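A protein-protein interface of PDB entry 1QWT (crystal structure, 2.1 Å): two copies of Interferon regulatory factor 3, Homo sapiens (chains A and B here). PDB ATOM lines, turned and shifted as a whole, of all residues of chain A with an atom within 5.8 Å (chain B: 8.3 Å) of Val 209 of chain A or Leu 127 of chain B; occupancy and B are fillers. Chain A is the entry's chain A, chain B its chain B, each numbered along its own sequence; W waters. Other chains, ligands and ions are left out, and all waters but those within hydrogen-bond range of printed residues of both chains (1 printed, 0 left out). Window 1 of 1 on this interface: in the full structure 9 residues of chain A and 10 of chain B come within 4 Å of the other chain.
The backbone carbonyl oxygen (O) of Ala 212 of chain A lies within hydrogen-bond range of the backbone NH (N) of Asn 130 of chain B, 2.8 Å away. OG of Ser 213 of chain A is in hydrogen-bond range of O of Leu 128 of chain B, 2.8 Å away. The backbone NH (N) of Glu 216 of chain A lies within hydrogen-bond range of the backbone carbonyl oxygen (O) of Gly 40 of chain B (2.8 Å). The backbone NH of Gln 42 of chain B lies within hydrogen-bond range of the side-chain carboxylate of Glu 216 of chain A (3.2 Å).
SD of Met 206 of chain A is in hydrogen-bond range of ND2 of Asn 217 of chain A (3.4 Å). OG of Ser 213 of chain A sits at hydrogen-bond distance from N of Leu 215 of chain A (3.0 Å). The indole nitrogen of Trp 173 of chain B is in hydrogen-bond range of the backbone carbonyl oxygen of Glu 125 of chain B. The guanidinium group of Arg 189 of chain B sits at hydrogen-bond distance from the backbone carbonyl oxygen of Pro 129 of chain B, 3.1 Å away.
Val 209 of chain A touches Leu 127 of chain B. Ala 212 of chain A touches Pro 129 of chain B (O to C, 3.7 Å). Ser 213 of chain A touches Leu 127 of chain B. C of Ser 213 of chain A touches ND2 of Asn 130 of chain B (3.4 Å). Leu 215 of chain A touches Gly 40 of chain B. Leu 215 of chain A touches Leu 127 of chain B (O to CD2, 3.7 Å). Leu 215 of chain A touches Leu 128 of chain B (CD1 to CB, 3.6 Å). CD1 of Leu 215 of chain A touches CZ3 of Trp 173 of chain B (3.7 Å). Glu 216 of chain A touches Leu 127 of chain B. CB of Asn 217 of chain A touches CD2 of Leu 127 of chain B (3.6 Å).
Val 209 of chain A touches just one residue of chain B: Leu 127 (3.5 Å). Leu 127 of chain B touches just these residues of chain A: Val 209, Ser 213, Leu 215, Glu 216 and Asn 217. No residue of chain B comes within 4 Å of Gly 210 of chain A. Of the printed residues of chain B, Asn 217 of chain A touches Leu 127 (3.6 Å). Of the printed residues of chain A, Pro 129 of chain B touches Ala 212 (3.7 Å). Of the printed residues of chain A, Gly 40 of chain B touches Leu 215 and Glu 216. Of the printed residues of chain A, Leu 128 of chain B touches Ser 213 and Leu 215. Of the printed residues of chain A, Phe 37 of chain B touches Leu 215 (3.99 Å). Glu 126 of chain B touches none of the printed residues of chain A. The nearest residue of chain B that does not touch Val 209 of chain A is Pro 129 of chain B (6.2 Å). The nearest printed residue of chain B that does not touch Ala 212 of chain A is Leu 128 of chain B (5.0 Å).
Hydrophobic or aromatic side chains of chain B that line the printed part of chain A: Phe 37, Leu 127, Leu 128 and Trp 173. Of the 13 printed residues of chain A, 6 touch a printed residue of chain B. Among the printed residues, no Asp or Glu carboxylate lies within 4 Å of a Lys or Arg side-chain nitrogen of the other chain.
No position is printed for both chains. Of the 15 pairs that touch across the chains among the printed residues, none has its exchanged pair printed and touching as well.
Water W1 lies within hydrogen-bond range of N of Glu 216 of chain A and O of Gly 40 of chain B.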
ATOM      1  N   VAL A 204      -3.841  20.032  12.816  1.00  0.00           N
ATOM      2  CA  VAL A 204      -4.604  21.048  13.539  1.00  0.00           C
ATOM      3  C   VAL A 204      -5.794  20.381  14.250  1.00  0.00           C
ATOM      4  O   VAL A 204      -6.071  20.663  15.411  1.00  0.00           O
ATOM      5  CB  VAL A 204      -5.124  22.150  12.583  1.00  0.00           C
ATOM      6  CG1 VAL A 204      -6.135  23.057  13.306  1.00  0.00           C
ATOM      7  CG2 VAL A 204      -3.954  22.986  12.082  1.00  0.00           C
ATOM      8  N   GLU A 205      -6.493  19.492  13.552  1.00  0.00           N
ATOM      9  CA  GLU A 205      -7.627  18.790  14.146  1.00  0.00           C
ATOM     10  C   GLU A 205      -7.174  17.979  15.355  1.00  0.00           C
ATOM     11  O   GLU A 205      -7.820  17.997  16.396  1.00  0.00           O
ATOM     12  CB  GLU A 205      -8.278  17.856  13.126  1.00  0.00           C
ATOM     13  CG  GLU A 205      -9.441  18.474  12.381  1.00  0.00           C
ATOM     14  CD  GLU A 205     -10.486  19.041  13.329  1.00  0.00           C
ATOM     15  OE1 GLU A 205     -10.367  20.228  13.707  1.00  0.00           O
ATOM     16  OE2 GLU A 205     -11.413  18.293  13.711  1.00  0.00           O
ATOM     17  N   MET A 206      -6.072  17.255  15.204  1.00  0.00           N
ATOM     18  CA  MET A 206      -5.526  16.457  16.298  1.00  0.00           C
ATOM     19  C   MET A 206      -5.343  17.344  17.526  1.00  0.00           C
ATOM     20  O   MET A 206      -5.716  16.972  18.635  1.00  0.00           O
ATOM     21  CB  MET A 206      -4.173  15.860  15.902  1.00  0.00           C
ATOM     22  CG  MET A 206      -3.434  15.174  17.061  1.00  0.00           C
ATOM     23  SD  MET A 206      -4.349  13.771  17.776  1.00  0.00           S
ATOM     24  CE  MET A 206      -2.997  12.815  18.523  1.00  0.00           C
ATOM     25  N   ALA A 207      -4.760  18.519  17.312  1.00  0.00           N
ATOM     26  CA  ALA A 207      -4.521  19.470  18.394  1.00  0.00           C
ATOM     27  C   ALA A 207      -5.820  20.027  18.979  1.00  0.00           C
ATOM     28  O   ALA A 207      -5.977  20.109  20.199  1.00  0.00           O
ATOM     29  CB  ALA A 207      -3.653  20.617  17.891  1.00  0.00           C
ATOM     30  N   ARG A 208      -6.743  20.415  18.105  1.00  0.00           N
ATOM     31  CA  ARG A 208      -8.020  20.979  18.535  1.00  0.00           C
ATOM     32  C   ARG A 208      -8.858  19.969  19.321  1.00  0.00           C
ATOM     33  O   ARG A 208      -9.352  20.270  20.409  1.00  0.00           O
ATOM     34  CB  ARG A 208      -8.814  21.466  17.318  1.00  0.00           C
ATOM     35  CG  ARG A 208     -10.166  22.089  17.655  1.00  0.00           C
ATOM     36  CD  ARG A 208     -10.953  22.457  16.395  1.00  0.00           C
ATOM     37  NE  ARG A 208     -11.565  21.295  15.747  1.00  0.00           N
ATOM     38  CZ  ARG A 208     -12.573  20.592  16.260  1.00  0.00           C
ATOM     39  NH1 ARG A 208     -13.095  20.926  17.436  1.00  0.00           N
ATOM     40  NH2 ARG A 208     -13.068  19.555  15.595  1.00  0.00           N
ATOM     41  N   VAL A 209      -9.003  18.766  18.772  1.00  0.00           N
ATOM     42  CA  VAL A 209      -9.793  17.723  19.414  1.00  0.00           C
ATOM     43  C   VAL A 209      -9.082  17.091  20.606  1.00  0.00           C
ATOM     44  O   VAL A 209      -9.652  16.994  21.692  1.00  0.00           O
ATOM     45  CB  VAL A 209     -10.162  16.622  18.400  1.00  0.00           C
ATOM     46  CG1 VAL A 209     -10.913  15.497  19.100  1.00  0.00           C
ATOM     47  CG2 VAL A 209     -11.019  17.220  17.282  1.00  0.00           C
ATOM     48  N   GLY A 210      -7.840  16.661  20.404  1.00  0.00           N
ATOM     49  CA  GLY A 210      -7.087  16.049  21.485  1.00  0.00           C
ATOM     50  C   GLY A 210      -6.861  16.960  22.682  1.00  0.00           C
ATOM     51  O   GLY A 210      -6.821  16.495  23.823  1.00  0.00           O
ATOM     52  N   GLY A 211      -6.724  18.259  22.436  1.00  0.00           N
ATOM     53  CA  GLY A 211      -6.489  19.194  23.526  1.00  0.00           C
ATOM     54  C   GLY A 211      -7.654  19.407  24.479  1.00  0.00           C
ATOM     55  O   GLY A 211      -7.463  19.821  25.624  1.00  0.00           O
ATOM     56  N   ALA A 212      -8.867  19.125  24.021  1.00  0.00           N
ATOM     57  CA  ALA A 212     -10.048  19.317  24.854  1.00  0.00           C
ATOM     58  C   ALA A 212     -10.595  18.018  25.448  1.00  0.00           C
ATOM     59  O   ALA A 212     -11.666  18.015  26.048  1.00  0.00           O
ATOM     60  CB  ALA A 212     -11.139  20.017  24.048  1.00  0.00           C
ATOM     61  N   SER A 213      -9.871  16.918  25.275  1.00  0.00           N
ATOM     62  CA  SER A 213     -10.308  15.628  25.810  1.00  0.00           C
ATOM     63  C   SER A 213      -9.167  14.839  26.447  1.00  0.00           C
ATOM     64  O   SER A 213      -8.023  14.932  26.012  1.00  0.00           O
ATOM     65  CB  SER A 213     -10.937  14.776  24.706  1.00  0.00           C
ATOM     66  OG  SER A 213     -11.199  13.467  25.185  1.00  0.00           O
ATOM     67  N   LEU A 215      -9.232  11.624  26.520  1.00  0.00           N
ATOM     68  CA  LEU A 215      -9.227  10.367  25.788  1.00  0.00           C
ATOM     69  C   LEU A 215      -8.245  10.409  24.622  1.00  0.00           C
ATOM     70  O   LEU A 215      -8.153  11.400  23.906  1.00  0.00           O
ATOM     71  CB  LEU A 215     -10.634  10.065  25.264  1.00  0.00           C
ATOM     72  CG  LEU A 215     -11.695   9.883  26.354  1.00  0.00           C
ATOM     73  CD1 LEU A 215     -13.081  10.147  25.786  1.00  0.00           C
ATOM     74  CD2 LEU A 215     -11.589   8.474  26.933  1.00  0.00           C
ATOM     75  N   GLU A 216      -7.521   9.313  24.447  1.00  0.00           N
ATOM     76  CA  GLU A 216      -6.540   9.150  23.379  1.00  0.00           C
ATOM     77  C   GLU A 216      -7.206   9.434  22.027  1.00  0.00           C
ATOM     78  O   GLU A 216      -8.235   8.843  21.715  1.00  0.00           O
ATOM     79  CB  GLU A 216      -6.046   7.707  23.418  1.00  0.00           C
ATOM     80  CG  GLU A 216      -4.692   7.441  22.837  1.00  0.00           C
ATOM     81  CD  GLU A 216      -4.182   6.087  23.280  1.00  0.00           C
ATOM     82  OE1 GLU A 216      -4.817   5.067  22.932  1.00  0.00           O
ATOM     83  OE2 GLU A 216      -3.157   6.044  23.992  1.00  0.00           O
ATOM     84  N   ASN A 217      -6.629  10.330  21.229  1.00  0.00           N
ATOM     85  CA  ASN A 217      -7.206  10.650  19.922  1.00  0.00           C
ATOM     86  C   ASN A 217      -6.394  10.030  18.785  1.00  0.00           C
ATOM     87  O   ASN A 217      -5.195   9.775  18.924  1.00  0.00           O
ATOM     88  CB  ASN A 217      -7.300  12.170  19.738  1.00  0.00           C
ATOM     89  CG  ASN A 217      -8.108  12.565  18.506  1.00  0.00           C
ATOM     90  OD1 ASN A 217      -9.075  11.902  18.144  1.00  0.00           O
ATOM     91  ND2 ASN A 217      -7.722  13.662  17.874  1.00  0.00           N
ATOM     92  N   PHE B  37     -11.961   2.318  26.646  1.00  0.00           N
ATOM     93  CA  PHE B  37     -10.789   3.062  27.091  1.00  0.00           C
ATOM     94  C   PHE B  37     -10.612   2.981  28.610  1.00  0.00           C
ATOM     95  O   PHE B  37     -11.574   3.146  29.362  1.00  0.00           O
ATOM     96  CB  PHE B  37     -10.904   4.547  26.710  1.00  0.00           C
ATOM     97  CG  PHE B  37     -11.133   4.799  25.239  1.00  0.00           C
ATOM     98  CD1 PHE B  37     -12.394   4.627  24.674  1.00  0.00           C
ATOM     99  CD2 PHE B  37     -10.090   5.240  24.427  1.00  0.00           C
ATOM    100  CE1 PHE B  37     -12.618   4.892  23.316  1.00  0.00           C
ATOM    101  CE2 PHE B  37     -10.299   5.509  23.066  1.00  0.00           C
ATOM    102  CZ  PHE B  37     -11.565   5.336  22.509  1.00  0.00           C
ATOM    103  N   GLY B  40      -8.328   6.751  29.778  1.00  0.00           N
ATOM    104  CA  GLY B  40      -8.139   7.448  28.514  1.00  0.00           C
ATOM    105  C   GLY B  40      -7.375   6.718  27.419  1.00  0.00           C
ATOM    106  O   GLY B  40      -7.217   7.238  26.320  1.00  0.00           O
ATOM    107  N   GLN B  42      -6.959   3.505  24.761  1.00  0.00           N
ATOM    108  CA  GLN B  42      -7.759   2.483  24.085  1.00  0.00           C
ATOM    109  C   GLN B  42      -7.196   1.113  24.406  1.00  0.00           C
ATOM    110  O   GLN B  42      -6.000   0.876  24.243  1.00  0.00           O
ATOM    111  CB  GLN B  42      -7.768   2.673  22.564  1.00  0.00           C
ATOM    112  CG  GLN B  42      -8.685   1.660  21.861  1.00  0.00           C
ATOM    113  CD  GLN B  42      -8.799   1.882  20.362  1.00  0.00           C
ATOM    114  OE1 GLN B  42      -8.991   3.005  19.905  1.00  0.00           O
ATOM    115  NE2 GLN B  42      -8.700   0.801  19.593  1.00  0.00           N
ATOM    116  N   SER B 124     -22.313  12.124  21.892  1.00  0.00           N
ATOM    117  CA  SER B 124     -21.331  13.179  21.631  1.00  0.00           C
ATOM    118  C   SER B 124     -20.560  12.942  20.325  1.00  0.00           C
ATOM    119  O   SER B 124     -21.041  12.228  19.440  1.00  0.00           O
ATOM    120  CB  SER B 124     -20.354  13.258  22.816  1.00  0.00           C
ATOM    121  OG  SER B 124     -19.403  14.297  22.661  1.00  0.00           O
ATOM    122  N   GLU B 125     -19.372  13.546  20.213  1.00  0.00           N
ATOM    123  CA  GLU B 125     -18.511  13.410  19.026  1.00  0.00           C
ATOM    124  C   GLU B 125     -17.754  12.080  19.058  1.00  0.00           C
ATOM    125  O   GLU B 125     -17.826  11.344  20.047  1.00  0.00           O
ATOM    126  CB  GLU B 125     -17.475  14.541  18.987  1.00  0.00           C
ATOM    127  CG  GLU B 125     -18.018  15.911  19.352  1.00  0.00           C
ATOM    128  CD  GLU B 125     -18.974  16.446  18.316  1.00  0.00           C
ATOM    129  OE1 GLU B 125     -19.807  17.310  18.670  1.00  0.00           O
ATOM    130  OE2 GLU B 125     -18.887  16.010  17.148  1.00  0.00           O
ATOM    131  N   GLU B 126     -17.004  11.790  17.995  1.00  0.00           N
ATOM    132  CA  GLU B 126     -16.221  10.557  17.924  1.00  0.00           C
ATOM    133  C   GLU B 126     -15.257  10.513  19.111  1.00  0.00           C
ATOM    134  O   GLU B 126     -14.786   9.446  19.493  1.00  0.00           O
ATOM    135  CB  GLU B 126     -15.444  10.472  16.598  1.00  0.00           C
ATOM    136  CG  GLU B 126     -16.300  10.193  15.343  1.00  0.00           C
ATOM    137  CD  GLU B 126     -16.578   8.703  15.101  1.00  0.00           C
ATOM    138  OE1 GLU B 126     -16.091   7.851  15.873  1.00  0.00           O
ATOM    139  OE2 GLU B 126     -17.284   8.380  14.124  1.00  0.00           O
ATOM    140  N   LEU B 127     -14.955  11.680  19.680  1.00  0.00           N
ATOM    141  CA  LEU B 127     -14.095  11.760  20.861  1.00  0.00           C
ATOM    142  C   LEU B 127     -14.834  12.625  21.887  1.00  0.00           C
ATOM    143  O   LEU B 127     -15.150  13.790  21.624  1.00  0.00           O
ATOM    144  CB  LEU B 127     -12.730  12.387  20.532  1.00  0.00           C
ATOM    145  CG  LEU B 127     -11.668  12.127  21.616  1.00  0.00           C
ATOM    146  CD1 LEU B 127     -11.344  10.631  21.644  1.00  0.00           C
ATOM    147  CD2 LEU B 127     -10.391  12.931  21.349  1.00  0.00           C
ATOM    148  N   LEU B 128     -15.126  12.044  23.046  1.00  0.00           N
ATOM    149  CA  LEU B 128     -15.843  12.739  24.110  1.00  0.00           C
ATOM    150  C   LEU B 128     -15.019  13.880  24.713  1.00  0.00           C
ATOM    151  O   LEU B 128     -13.962  13.654  25.295  1.00  0.00           O
ATOM    152  CB  LEU B 128     -16.213  11.747  25.216  1.00  0.00           C
ATOM    153  CG  LEU B 128     -17.050  12.279  26.381  1.00  0.00           C
ATOM    154  CD1 LEU B 128     -18.467  12.581  25.891  1.00  0.00           C
ATOM    155  CD2 LEU B 128     -17.087  11.233  27.507  1.00  0.00           C
ATOM    156  N   PRO B 129     -15.505  15.123  24.590  1.00  0.00           N
ATOM    157  CA  PRO B 129     -14.804  16.297  25.130  1.00  0.00           C
ATOM    158  C   PRO B 129     -14.910  16.393  26.656  1.00  0.00           C
ATOM    159  O   PRO B 129     -15.895  15.946  27.238  1.00  0.00           O
ATOM    160  CB  PRO B 129     -15.514  17.474  24.451  1.00  0.00           C
ATOM    161  CG  PRO B 129     -16.205  16.848  23.238  1.00  0.00           C
ATOM    162  CD  PRO B 129     -16.662  15.527  23.778  1.00  0.00           C
ATOM    163  N   ASN B 130     -13.895  16.959  27.306  1.00  0.00           N
ATOM    164  CA  ASN B 130     -13.952  17.124  28.757  1.00  0.00           C
ATOM    165  C   ASN B 130     -14.822  18.348  29.021  1.00  0.00           C
ATOM    166  O   ASN B 130     -14.823  19.286  28.230  1.00  0.00           O
ATOM    167  CB  ASN B 130     -12.561  17.368  29.357  1.00  0.00           C
ATOM    168  CG  ASN B 130     -11.658  16.155  29.264  1.00  0.00           C
ATOM    169  OD1 ASN B 130     -12.122  15.014  29.258  1.00  0.00           O
ATOM    170  ND2 ASN B 130     -10.355  16.398  29.216  1.00  0.00           N
ATOM    171  N   TYR B 170     -23.626  11.057  16.586  1.00  0.00           N
ATOM    172  CA  TYR B 170     -24.095   9.670  16.575  1.00  0.00           C
ATOM    173  C   TYR B 170     -23.302   8.729  17.478  1.00  0.00           C
ATOM    174  O   TYR B 170     -23.587   7.530  17.526  1.00  0.00           O
ATOM    175  CB  TYR B 170     -24.056   9.133  15.139  1.00  0.00           C
ATOM    176  CG  TYR B 170     -22.697   9.287  14.490  1.00  0.00           C
ATOM    177  CD1 TYR B 170     -21.644   8.428  14.809  1.00  0.00           C
ATOM    178  CD2 TYR B 170     -22.441  10.344  13.616  1.00  0.00           C
ATOM    179  CE1 TYR B 170     -20.368   8.620  14.275  1.00  0.00           C
ATOM    180  CE2 TYR B 170     -21.170  10.548  13.080  1.00  0.00           C
ATOM    181  CZ  TYR B 170     -20.139   9.686  13.413  1.00  0.00           C
ATOM    182  OH  TYR B 170     -18.886   9.893  12.881  1.00  0.00           O
ATOM    183  N   ALA B 171     -22.317   9.258  18.196  1.00  0.00           N
ATOM    184  CA  ALA B 171     -21.496   8.414  19.060  1.00  0.00           C
ATOM    185  C   ALA B 171     -22.021   8.336  20.487  1.00  0.00           C
ATOM    186  O   ALA B 171     -22.198   9.364  21.152  1.00  0.00           O
ATOM    187  CB  ALA B 171     -20.052   8.921  19.066  1.00  0.00           C
ATOM    188  N   TRP B 173     -21.538   7.325  24.361  1.00  0.00           N
ATOM    189  CA  TRP B 173     -20.477   7.119  25.328  1.00  0.00           C
ATOM    190  C   TRP B 173     -21.058   6.661  26.649  1.00  0.00           C
ATOM    191  O   TRP B 173     -21.955   7.294  27.201  1.00  0.00           O
ATOM    192  CB  TRP B 173     -19.676   8.404  25.539  1.00  0.00           C
ATOM    193  CG  TRP B 173     -18.776   8.715  24.396  1.00  0.00           C
ATOM    194  CD1 TRP B 173     -19.090   9.418  23.263  1.00  0.00           C
ATOM    195  CD2 TRP B 173     -17.406   8.325  24.263  1.00  0.00           C
ATOM    196  NE1 TRP B 173     -17.994   9.496  22.438  1.00  0.00           N
ATOM    197  CE2 TRP B 173     -16.946   8.832  23.024  1.00  0.00           C
ATOM    198  CE3 TRP B 173     -16.519   7.597  25.070  1.00  0.00           C
ATOM    199  CZ2 TRP B 173     -15.638   8.635  22.573  1.00  0.00           C
ATOM    200  CZ3 TRP B 173     -15.216   7.400  24.623  1.00  0.00           C
ATOM    201  CH2 TRP B 173     -14.788   7.920  23.384  1.00  0.00           C
ATOM    202  N   ARG B 189     -13.573   9.595  34.653  1.00  0.00           N
ATOM    203  CA  ARG B 189     -13.821   8.813  33.443  1.00  0.00           C
ATOM    204  C   ARG B 189     -12.762   7.743  33.173  1.00  0.00           C
ATOM    205  O   ARG B 189     -12.216   7.660  32.076  1.00  0.00           O
ATOM    206  CB  ARG B 189     -13.931   9.758  32.236  1.00  0.00           C
ATOM    207  CG  ARG B 189     -15.009  10.812  32.413  1.00  0.00           C
ATOM    208  CD  ARG B 189     -15.066  11.836  31.284  1.00  0.00           C
ATOM    209  NE  ARG B 189     -16.048  12.864  31.618  1.00  0.00           N
ATOM    210  CZ  ARG B 189     -16.331  13.927  30.872  1.00  0.00           C
ATOM    211  NH1 ARG B 189     -15.709  14.131  29.716  1.00  0.00           N
ATOM    212  NH2 ARG B 189     -17.249  14.788  31.289  1.00  0.00           N
ATOM    213  N   LYS B 194     -17.138   3.560  23.985  1.00  0.00           N
ATOM    214  CA  LYS B 194     -17.795   4.236  22.886  1.00  0.00           C
ATOM    215  C   LYS B 194     -18.507   3.219  22.011  1.00  0.00           C
ATOM    216  O   LYS B 194     -17.954   2.166  21.685  1.00  0.00           O
ATOM    217  CB  LYS B 194     -16.785   5.008  22.023  1.00  0.00           C
ATOM    218  CG  LYS B 194     -17.433   5.609  20.763  1.00  0.00           C
ATOM    219  CD  LYS B 194     -16.564   6.623  20.033  1.00  0.00           C
ATOM    220  CE  LYS B 194     -15.434   5.974  19.271  1.00  0.00           C
ATOM    221  NZ  LYS B 194     -14.833   6.938  18.288  1.00  0.00           N
ATOM    222  N   VAL B 196     -20.560   3.052  18.395  1.00  0.00           N
ATOM    223  CA  VAL B 196     -20.960   3.750  17.192  1.00  0.00           C
ATOM    224  C   VAL B 196     -21.682   2.876  16.179  1.00  0.00           C
ATOM    225  O   VAL B 196     -21.153   1.854  15.732  1.00  0.00           O
ATOM    226  CB  VAL B 196     -19.743   4.372  16.473  1.00  0.00           C
ATOM    227  CG1 VAL B 196     -20.140   4.803  15.062  1.00  0.00           C
ATOM    228  CG2 VAL B 196     -19.219   5.559  17.254  1.00  0.00           C
ATOM    229  N   ARG B 201     -22.360   6.743  11.024  1.00  0.00           N
ATOM    230  CA  ARG B 201     -21.086   7.370  10.694  1.00  0.00           C
ATOM    231  C   ARG B 201     -21.025   7.502   9.171  1.00  0.00           C
ATOM    232  O   ARG B 201     -20.587   8.519   8.639  1.00  0.00           O
ATOM    233  CB  ARG B 201     -19.925   6.498  11.184  1.00  0.00           C
ATOM    234  CG  ARG B 201     -18.556   6.924  10.674  1.00  0.00           C
ATOM    235  CD  ARG B 201     -17.487   5.949  11.138  1.00  0.00           C
ATOM    236  NE  ARG B 201     -17.136   6.127  12.549  1.00  0.00           N
ATOM    237  CZ  ARG B 201     -16.638   5.168  13.322  1.00  0.00           C
ATOM    238  NH1 ARG B 201     -16.444   3.953  12.830  1.00  0.00           N
ATOM    239  NH2 ARG B 201     -16.302   5.432  14.580  1.00  0.00           N
HETATM  240  O   HOH W   1      -5.199  10.053  26.741  1.00  0.00           O
